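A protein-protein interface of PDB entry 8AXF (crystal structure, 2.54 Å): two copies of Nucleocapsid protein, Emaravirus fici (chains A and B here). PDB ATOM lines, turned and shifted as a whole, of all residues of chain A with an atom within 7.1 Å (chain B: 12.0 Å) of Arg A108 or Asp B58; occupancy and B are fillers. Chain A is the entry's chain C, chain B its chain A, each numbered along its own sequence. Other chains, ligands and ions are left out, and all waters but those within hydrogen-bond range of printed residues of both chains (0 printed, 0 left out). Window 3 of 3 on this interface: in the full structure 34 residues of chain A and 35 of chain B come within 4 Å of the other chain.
His A91 touches Glu B60 (CE1 to O, 3.7 Å). Val B61 touches His A91. Arg A105 touches Pro B56. Asn A106 touches Leu B54 (OD1 to CD2, 3.2 Å). C of Leu A107 touches CB of Pro B56, 3.7 Å away. Leu A107 touches Ile B57. Leu A107 touches Val B59 (CD2 to CG2, 3.7 Å). Pro B56 touches Arg A108. N of Val B59 touches O of Arg A108 (3.5 Å). Leu A109 touches Val B59.
No position is printed for both chains.
Arg A108 touches four residues of chain B. Leu A107 touches just these residues of chain B: Pro B56 (3.7 Å), Ile B57 (3.5 Å) and Val B59 (3.7 Å). Of the printed residues of chain B, Ile A110 touches Val B61. Phe A116 touches none of the printed residues of chain B. No residue of chain B comes within 4 Å of Val A118. No residue of chain B comes within 4 Å of Val A119. Of the printed residues of chain A, Glu B60 touches His A91 (3.7 Å). Of the printed residues of chain B, Asn A106 touches Leu B54, Lys B55, Pro B56 and Ile B57. Of the printed residues of chain A, Leu B54 touches Asn A106. Glu A115 touches none of the printed residues of chain B. The nearest residue of chain A that does not touch Asp B58 is Leu A107 (6.1 Å). The nearest printed residue of chain B that does not touch Asn A106 is Asp B58 (6.5 Å).
The guanidinium group of Arg A105 sits at hydrogen-bond distance from the backbone carbonyl oxygen of Lys B55, at 3.0 Å. N of Ile B57 is in hydrogen-bond range of O of Asn A106, 3.3 Å away. O of Ile B57 lies within hydrogen-bond range of N of Arg A108, at 3.3 Å. The side-chain carboxylate (OD1) of Asp B58 lies within salt-bridge range of the guanidinium group (NE) of Arg A108 (3.6 Å).
Of the 14 printed residues of chain A, 7 touch a printed residue of chain B. Hydrophobic or aromatic side chains of chain A within 4 Å of the printed part of chain B: His A91, Leu A107, Leu A109 and Ile A110. Of the 10 printed residues of chain B, 8 touch a printed residue of chain A. Printed residues of chain B that touch a printed residue of chain A: Leu B54, Lys B55, Pro B56, Ile B57, Asp B58, Val B59, Glu B60 and Val B61. Hydrophobic or aromatic side chains of chain B within 4 Å of the printed part of chain A: Leu B54, Pro B56, Ile B57, Val B59 and Val B61. Among the printed residues, 18 pairs touch across the chains. Among the printed residues, Asp or Glu carboxylates within 4 Å of a Lys or Arg side-chain nitrogen of the other chain: Arg A108 with Asp B58 (3.6 Å).
O of Ile A110 lies within hydrogen-bond range of NE2 of His A91. O of Leu A107 lies within hydrogen-bond range of N of Val A119 (2.9 Å). O of Leu A117 lies within hydrogen-bond range of N of Leu A109 (2.6 Å).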
ATOM      1  N   HIS A  91      13.307  -2.321   9.931  1.00  0.00           N
ATOM      2  CA  HIS A  91      12.894  -3.667  10.313  1.00  0.00           C
ATOM      3  C   HIS A  91      13.710  -4.732   9.593  1.00  0.00           C
ATOM      4  O   HIS A  91      13.983  -5.793  10.169  1.00  0.00           O
ATOM      5  CB  HIS A  91      11.404  -3.860  10.032  1.00  0.00           C
ATOM      6  CG  HIS A  91      10.519  -2.956  10.834  1.00  0.00           C
ATOM      7  ND1 HIS A  91      10.735  -2.700  12.171  1.00  0.00           N
ATOM      8  CD2 HIS A  91       9.424  -2.240  10.485  1.00  0.00           C
ATOM      9  CE1 HIS A  91       9.807  -1.870  12.613  1.00  0.00           C
ATOM     10  NE2 HIS A  91       9.000  -1.575  11.610  1.00  0.00           N
ATOM     11  N   LEU A 102      10.470 -13.789  16.880  1.00  0.00           N
ATOM     12  CA  LEU A 102       9.272 -14.411  16.330  1.00  0.00           C
ATOM     13  C   LEU A 102       9.072 -15.811  16.896  1.00  0.00           C
ATOM     14  O   LEU A 102       7.934 -16.233  17.131  1.00  0.00           O
ATOM     15  CB  LEU A 102       9.348 -14.444  14.802  1.00  0.00           C
ATOM     16  CG  LEU A 102       8.152 -15.053  14.064  1.00  0.00           C
ATOM     17  CD1 LEU A 102       6.942 -14.140  14.183  1.00  0.00           C
ATOM     18  CD2 LEU A 102       8.492 -15.323  12.604  1.00  0.00           C
ATOM     19  N   ARG A 105       7.148 -15.518  20.408  1.00  0.00           N
ATOM     20  CA  ARG A 105       5.794 -15.051  20.176  1.00  0.00           C
ATOM     21  C   ARG A 105       5.764 -14.371  18.815  1.00  0.00           C
ATOM     22  O   ARG A 105       6.783 -13.855  18.343  1.00  0.00           O
ATOM     23  CB  ARG A 105       5.328 -14.075  21.266  1.00  0.00           C
ATOM     24  CG  ARG A 105       5.461 -14.581  22.692  1.00  0.00           C
ATOM     25  CD  ARG A 105       5.265 -13.468  23.718  1.00  0.00           C
ATOM     26  NE  ARG A 105       3.892 -13.379  24.209  1.00  0.00           N
ATOM     27  CZ  ARG A 105       2.951 -12.604  23.677  1.00  0.00           C
ATOM     28  NH1 ARG A 105       3.226 -11.850  22.622  1.00  0.00           N
ATOM     29  NH2 ARG A 105       1.732 -12.585  24.198  1.00  0.00           N
ATOM     30  N   ASN A 106       4.591 -14.369  18.189  1.00  0.00           N
ATOM     31  CA  ASN A 106       4.493 -13.772  16.874  1.00  0.00           C
ATOM     32  C   ASN A 106       4.358 -12.255  17.000  1.00  0.00           C
ATOM     33  O   ASN A 106       4.060 -11.715  18.072  1.00  0.00           O
ATOM     34  CB  ASN A 106       3.314 -14.346  16.102  1.00  0.00           C
ATOM     35  CG  ASN A 106       3.355 -15.862  16.004  1.00  0.00           C
ATOM     36  OD1 ASN A 106       2.328 -16.512  15.843  1.00  0.00           O
ATOM     37  ND2 ASN A 106       4.559 -16.437  16.121  1.00  0.00           N
ATOM     38  N   LEU A 107       4.620 -11.560  15.892  1.00  0.00           N
ATOM     39  CA  LEU A 107       4.983 -10.150  15.927  1.00  0.00           C
ATOM     40  C   LEU A 107       4.014  -9.298  15.112  1.00  0.00           C
ATOM     41  O   LEU A 107       3.235  -9.797  14.289  1.00  0.00           O
ATOM     42  CB  LEU A 107       6.410  -9.946  15.399  1.00  0.00           C
ATOM     43  CG  LEU A 107       7.556 -10.713  16.079  1.00  0.00           C
ATOM     44  CD1 LEU A 107       8.868 -10.486  15.343  1.00  0.00           C
ATOM     45  CD2 LEU A 107       7.693 -10.298  17.523  1.00  0.00           C
ATOM     46  N   ARG A 108       4.114  -7.984  15.331  1.00  0.00           N
ATOM     47  CA  ARG A 108       3.333  -6.975  14.627  1.00  0.00           C
ATOM     48  C   ARG A 108       4.252  -5.815  14.284  1.00  0.00           C
ATOM     49  O   ARG A 108       4.948  -5.293  15.161  1.00  0.00           O
ATOM     50  CB  ARG A 108       2.148  -6.487  15.475  1.00  0.00           C
ATOM     51  CG  ARG A 108       1.053  -5.774  14.688  1.00  0.00           C
ATOM     52  CD  ARG A 108       1.152  -4.250  14.782  1.00  0.00           C
ATOM     53  NE  ARG A 108       0.322  -3.684  15.847  1.00  0.00           N
ATOM     54  CZ  ARG A 108       0.317  -2.397  16.193  1.00  0.00           C
ATOM     55  NH1 ARG A 108       1.099  -1.533  15.560  1.00  0.00           N
ATOM     56  NH2 ARG A 108      -0.468  -1.972  17.174  1.00  0.00           N
ATOM     57  N   LEU A 109       4.252  -5.414  13.014  1.00  0.00           N
ATOM     58  CA  LEU A 109       5.218  -4.459  12.485  1.00  0.00           C
ATOM     59  C   LEU A 109       4.495  -3.336  11.762  1.00  0.00           C
ATOM     60  O   LEU A 109       3.860  -3.571  10.726  1.00  0.00           O
ATOM     61  CB  LEU A 109       6.196  -5.140  11.520  1.00  0.00           C
ATOM     62  CG  LEU A 109       7.418  -5.825  12.128  1.00  0.00           C
ATOM     63  CD1 LEU A 109       8.051  -4.944  13.197  1.00  0.00           C
ATOM     64  CD2 LEU A 109       7.081  -7.201  12.672  1.00  0.00           C
ATOM     65  N   ILE A 110       4.607  -2.120  12.292  1.00  0.00           N
ATOM     66  CA  ILE A 110       4.144  -0.938  11.575  1.00  0.00           C
ATOM     67  C   ILE A 110       5.108  -0.645  10.437  1.00  0.00           C
ATOM     68  O   ILE A 110       6.321  -0.532  10.640  1.00  0.00           O
ATOM     69  CB  ILE A 110       4.013   0.273  12.512  1.00  0.00           C
ATOM     70  CG1 ILE A 110       5.222   0.404  13.439  1.00  0.00           C
ATOM     71  CG2 ILE A 110       2.711   0.201  13.273  1.00  0.00           C
ATOM     72  CD1 ILE A 110       5.240   1.721  14.197  1.00  0.00           C
ATOM     73  N   ASN A 114      -0.403   4.242   9.123  1.00  0.00           N
ATOM     74  CA  ASN A 114      -1.492   3.420   9.630  1.00  0.00           C
ATOM     75  C   ASN A 114      -1.405   1.958   9.228  1.00  0.00           C
ATOM     76  O   ASN A 114      -1.959   1.116   9.930  1.00  0.00           O
ATOM     77  CB  ASN A 114      -2.855   3.979   9.193  1.00  0.00           C
ATOM     78  CG  ASN A 114      -2.904   4.341   7.715  1.00  0.00           C
ATOM     79  OD1 ASN A 114      -2.215   3.750   6.879  1.00  0.00           O
ATOM     80  ND2 ASN A 114      -3.737   5.321   7.388  1.00  0.00           N
ATOM     81  N   GLU A 115      -0.719   1.631   8.136  1.00  0.00           N
ATOM     82  CA  GLU A 115      -0.659   0.248   7.689  1.00  0.00           C
ATOM     83  C   GLU A 115       0.358  -0.545   8.500  1.00  0.00           C
ATOM     84  O   GLU A 115       1.421  -0.036   8.881  1.00  0.00           O
ATOM     85  CB  GLU A 115      -0.314   0.170   6.213  1.00  0.00           C
ATOM     86  CG  GLU A 115      -1.536   0.208   5.329  1.00  0.00           C
ATOM     87  CD  GLU A 115      -2.581  -0.791   5.776  1.00  0.00           C
ATOM     88  OE1 GLU A 115      -2.269  -2.001   5.821  1.00  0.00           O
ATOM     89  OE2 GLU A 115      -3.711  -0.359   6.095  1.00  0.00           O
ATOM     90  N   PHE A 116       0.018  -1.808   8.754  1.00  0.00           N
ATOM     91  CA  PHE A 116       0.791  -2.688   9.611  1.00  0.00           C
ATOM     92  C   PHE A 116       0.879  -4.065   8.972  1.00  0.00           C
ATOM     93  O   PHE A 116       0.174  -4.378   8.006  1.00  0.00           O
ATOM     94  CB  PHE A 116       0.160  -2.781  11.007  1.00  0.00           C
ATOM     95  CG  PHE A 116      -1.342  -2.807  10.997  1.00  0.00           C
ATOM     96  CD1 PHE A 116      -2.036  -3.856  10.412  1.00  0.00           C
ATOM     97  CD2 PHE A 116      -2.067  -1.770  11.557  1.00  0.00           C
ATOM     98  CE1 PHE A 116      -3.423  -3.874  10.397  1.00  0.00           C
ATOM     99  CE2 PHE A 116      -3.452  -1.782  11.548  1.00  0.00           C
ATOM    100  CZ  PHE A 116      -4.130  -2.834  10.967  1.00  0.00           C
ATOM    101  N   LEU A 117       1.732  -4.904   9.556  1.00  0.00           N
ATOM    102  CA  LEU A 117       1.880  -6.294   9.153  1.00  0.00           C
ATOM    103  C   LEU A 117       2.102  -7.149  10.389  1.00  0.00           C
ATOM    104  O   LEU A 117       2.876  -6.782  11.278  1.00  0.00           O
ATOM    105  CB  LEU A 117       3.047  -6.489   8.169  1.00  0.00           C
ATOM    106  CG  LEU A 117       2.822  -6.025   6.727  1.00  0.00           C
ATOM    107  CD1 LEU A 117       4.149  -5.814   6.010  1.00  0.00           C
ATOM    108  CD2 LEU A 117       1.954  -7.020   5.963  1.00  0.00           C
ATOM    109  N   VAL A 118       1.410  -8.282  10.446  1.00  0.00           N
ATOM    110  CA  VAL A 118       1.558  -9.249  11.525  1.00  0.00           C
ATOM    111  C   VAL A 118       2.325 -10.446  10.986  1.00  0.00           C
ATOM    112  O   VAL A 118       1.895 -11.088  10.020  1.00  0.00           O
ATOM    113  CB  VAL A 118       0.194  -9.676  12.086  1.00  0.00           C
ATOM    114  CG1 VAL A 118       0.342 -10.945  12.895  1.00  0.00           C
ATOM    115  CG2 VAL A 118      -0.394  -8.564  12.936  1.00  0.00           C
ATOM    116  N   VAL A 119       3.466 -10.741  11.602  1.00  0.00           N
ATOM    117  CA  VAL A 119       4.306 -11.866  11.213  1.00  0.00           C
ATOM    118  C   VAL A 119       4.016 -13.035  12.142  1.00  0.00           C
ATOM    119  O   VAL A 119       3.888 -12.858  13.360  1.00  0.00           O
ATOM    120  CB  VAL A 119       5.797 -11.482  11.247  1.00  0.00           C
ATOM    121  CG1 VAL A 119       6.643 -12.610  10.695  1.00  0.00           C
ATOM    122  CG2 VAL A 119       6.026 -10.199  10.461  1.00  0.00           C
ATOM    123  N   SER B  52      -5.565 -15.707  13.862  1.00  0.00           N
ATOM    124  CA  SER B  52      -6.441 -16.444  14.755  1.00  0.00           C
ATOM    125  C   SER B  52      -5.726 -16.862  16.041  1.00  0.00           C
ATOM    126  O   SER B  52      -4.749 -17.616  16.012  1.00  0.00           O
ATOM    127  CB  SER B  52      -7.009 -17.683  14.046  1.00  0.00           C
ATOM    128  OG  SER B  52      -7.762 -18.489  14.931  1.00  0.00           O
ATOM    129  N   LEU B  54      -3.845 -15.289  18.284  1.00  0.00           N
ATOM    130  CA  LEU B  54      -2.444 -14.918  18.390  1.00  0.00           C
ATOM    131  C   LEU B  54      -2.348 -13.524  18.984  1.00  0.00           C
ATOM    132  O   LEU B  54      -2.989 -12.585  18.498  1.00  0.00           O
ATOM    133  CB  LEU B  54      -1.742 -14.972  17.030  1.00  0.00           C
ATOM    134  CG  LEU B  54      -0.234 -14.684  16.981  1.00  0.00           C
ATOM    135  CD1 LEU B  54       0.072 -13.190  16.843  1.00  0.00           C
ATOM    136  CD2 LEU B  54       0.493 -15.274  18.192  1.00  0.00           C
ATOM    137  N   LYS B  55      -1.536 -13.401  20.029  1.00  0.00           N
ATOM    138  CA  LYS B  55      -1.189 -12.115  20.599  1.00  0.00           C
ATOM    139  C   LYS B  55       0.176 -11.702  20.086  1.00  0.00           C
ATOM    140  O   LYS B  55       1.172 -12.352  20.432  1.00  0.00           O
ATOM    141  CB  LYS B  55      -1.174 -12.183  22.119  1.00  0.00           C
ATOM    142  CG  LYS B  55      -0.923 -10.827  22.766  1.00  0.00           C
ATOM    143  CD  LYS B  55      -1.962  -9.794  22.317  1.00  0.00           C
ATOM    144  CE  LYS B  55      -1.695  -8.442  22.974  1.00  0.00           C
ATOM    145  NZ  LYS B  55      -0.323  -7.931  22.694  1.00  0.00           N
ATOM    146  N   PRO B  56       0.273 -10.661  19.270  1.00  0.00           N
ATOM    147  CA  PRO B  56       1.574 -10.150  18.845  1.00  0.00           C
ATOM    148  C   PRO B  56       2.142  -9.190  19.884  1.00  0.00           C
ATOM    149  O   PRO B  56       1.453  -8.721  20.790  1.00  0.00           O
ATOM    150  CB  PRO B  56       1.236  -9.410  17.546  1.00  0.00           C
ATOM    151  CG  PRO B  56      -0.139  -8.869  17.809  1.00  0.00           C
ATOM    152  CD  PRO B  56      -0.840  -9.862  18.734  1.00  0.00           C
ATOM    153  N   ILE B  57       3.426  -8.898  19.719  1.00  0.00           N
ATOM    154  CA  ILE B  57       4.101  -7.841  20.461  1.00  0.00           C
ATOM    155  C   ILE B  57       4.595  -6.789  19.478  1.00  0.00           C
ATOM    156  O   ILE B  57       5.010  -7.101  18.352  1.00  0.00           O
ATOM    157  CB  ILE B  57       5.260  -8.351  21.338  1.00  0.00           C
ATOM    158  CG1 ILE B  57       6.143  -9.335  20.565  1.00  0.00           C
ATOM    159  CG2 ILE B  57       4.704  -8.979  22.595  1.00  0.00           C
ATOM    160  CD1 ILE B  57       7.606  -9.242  20.968  1.00  0.00           C
ATOM    161  N   ASP B  58       4.550  -5.525  19.926  1.00  0.00           N
ATOM    162  CA  ASP B  58       4.754  -4.364  19.064  1.00  0.00           C
ATOM    163  C   ASP B  58       6.243  -4.044  19.017  1.00  0.00           C
ATOM    164  O   ASP B  58       6.796  -3.360  19.883  1.00  0.00           O
ATOM    165  CB  ASP B  58       3.936  -3.185  19.560  1.00  0.00           C
ATOM    166  CG  ASP B  58       2.447  -3.483  19.580  1.00  0.00           C
ATOM    167  OD1 ASP B  58       2.016  -4.443  18.902  1.00  0.00           O
ATOM    168  OD2 ASP B  58       1.708  -2.763  20.276  1.00  0.00           O
ATOM    169  N   VAL B  59       6.900  -4.576  17.990  1.00  0.00           N
ATOM    170  CA  VAL B  59       8.329  -4.374  17.804  1.00  0.00           C
ATOM    171  C   VAL B  59       8.603  -2.919  17.456  1.00  0.00           C
ATOM    172  O   VAL B  59       7.881  -2.304  16.658  1.00  0.00           O
ATOM    173  CB  VAL B  59       8.843  -5.314  16.704  1.00  0.00           C
ATOM    174  CG1 VAL B  59      10.344  -5.378  16.752  1.00  0.00           C
ATOM    175  CG2 VAL B  59       8.203  -6.687  16.852  1.00  0.00           C
ATOM    176  N   GLU B  60       9.649  -2.364  18.061  1.00  0.00           N
ATOM    177  CA  GLU B  60      10.035  -0.983  17.851  1.00  0.00           C
ATOM    178  C   GLU B  60      10.726  -0.803  16.506  1.00  0.00           C
ATOM    179  O   GLU B  60      11.392  -1.704  15.988  1.00  0.00           O
ATOM    180  CB  GLU B  60      10.971  -0.510  18.969  1.00  0.00           C
ATOM    181  CG  GLU B  60      10.261   0.136  20.151  1.00  0.00           C
ATOM    182  CD  GLU B  60       9.659   1.493  19.800  1.00  0.00           C
ATOM    183  OE1 GLU B  60       8.814   2.001  20.575  1.00  0.00           O
ATOM    184  OE2 GLU B  60      10.043   2.060  18.753  1.00  0.00           O
ATOM    185  N   VAL B  61      10.565   0.394  15.952  1.00  0.00           N
ATOM    186  CA  VAL B  61      11.250   0.794  14.723  1.00  0.00           C
ATOM    187  C   VAL B  61      12.591   1.378  15.156  1.00  0.00           C
ATOM    188  O   VAL B  61      12.704   2.559  15.496  1.00  0.00           O
ATOM    189  CB  VAL B  61      10.428   1.788  13.909  1.00  0.00           C
ATOM    190  CG1 VAL B  61      11.083   2.029  12.568  1.00  0.00           C
ATOM    191  CG2 VAL B  61       9.014   1.289  13.745  1.00  0.00           C
ATOM    192  N   GLN B  62      13.620   0.535  15.153  1.00  0.00           N
ATOM    193  CA  GLN B  62      14.975   0.947  15.492  1.00  0.00           C
ATOM    194  C   GLN B  62      15.917   0.382  14.444  1.00  0.00           C
ATOM    195  O   GLN B  62      15.974  -0.837  14.244  1.00  0.00           O
ATOM    196  CB  GLN B  62      15.383   0.482  16.896  1.00  0.00           C
ATOM    197  CG  GLN B  62      14.880  -0.894  17.280  1.00  0.00           C
ATOM    198  CD  GLN B  62      15.531  -1.430  18.544  1.00  0.00           C
ATOM    199  OE1 GLN B  62      16.563  -0.928  18.991  1.00  0.00           O
ATOM    200  NE2 GLN B  62      14.927  -2.459  19.125  1.00  0.00           N
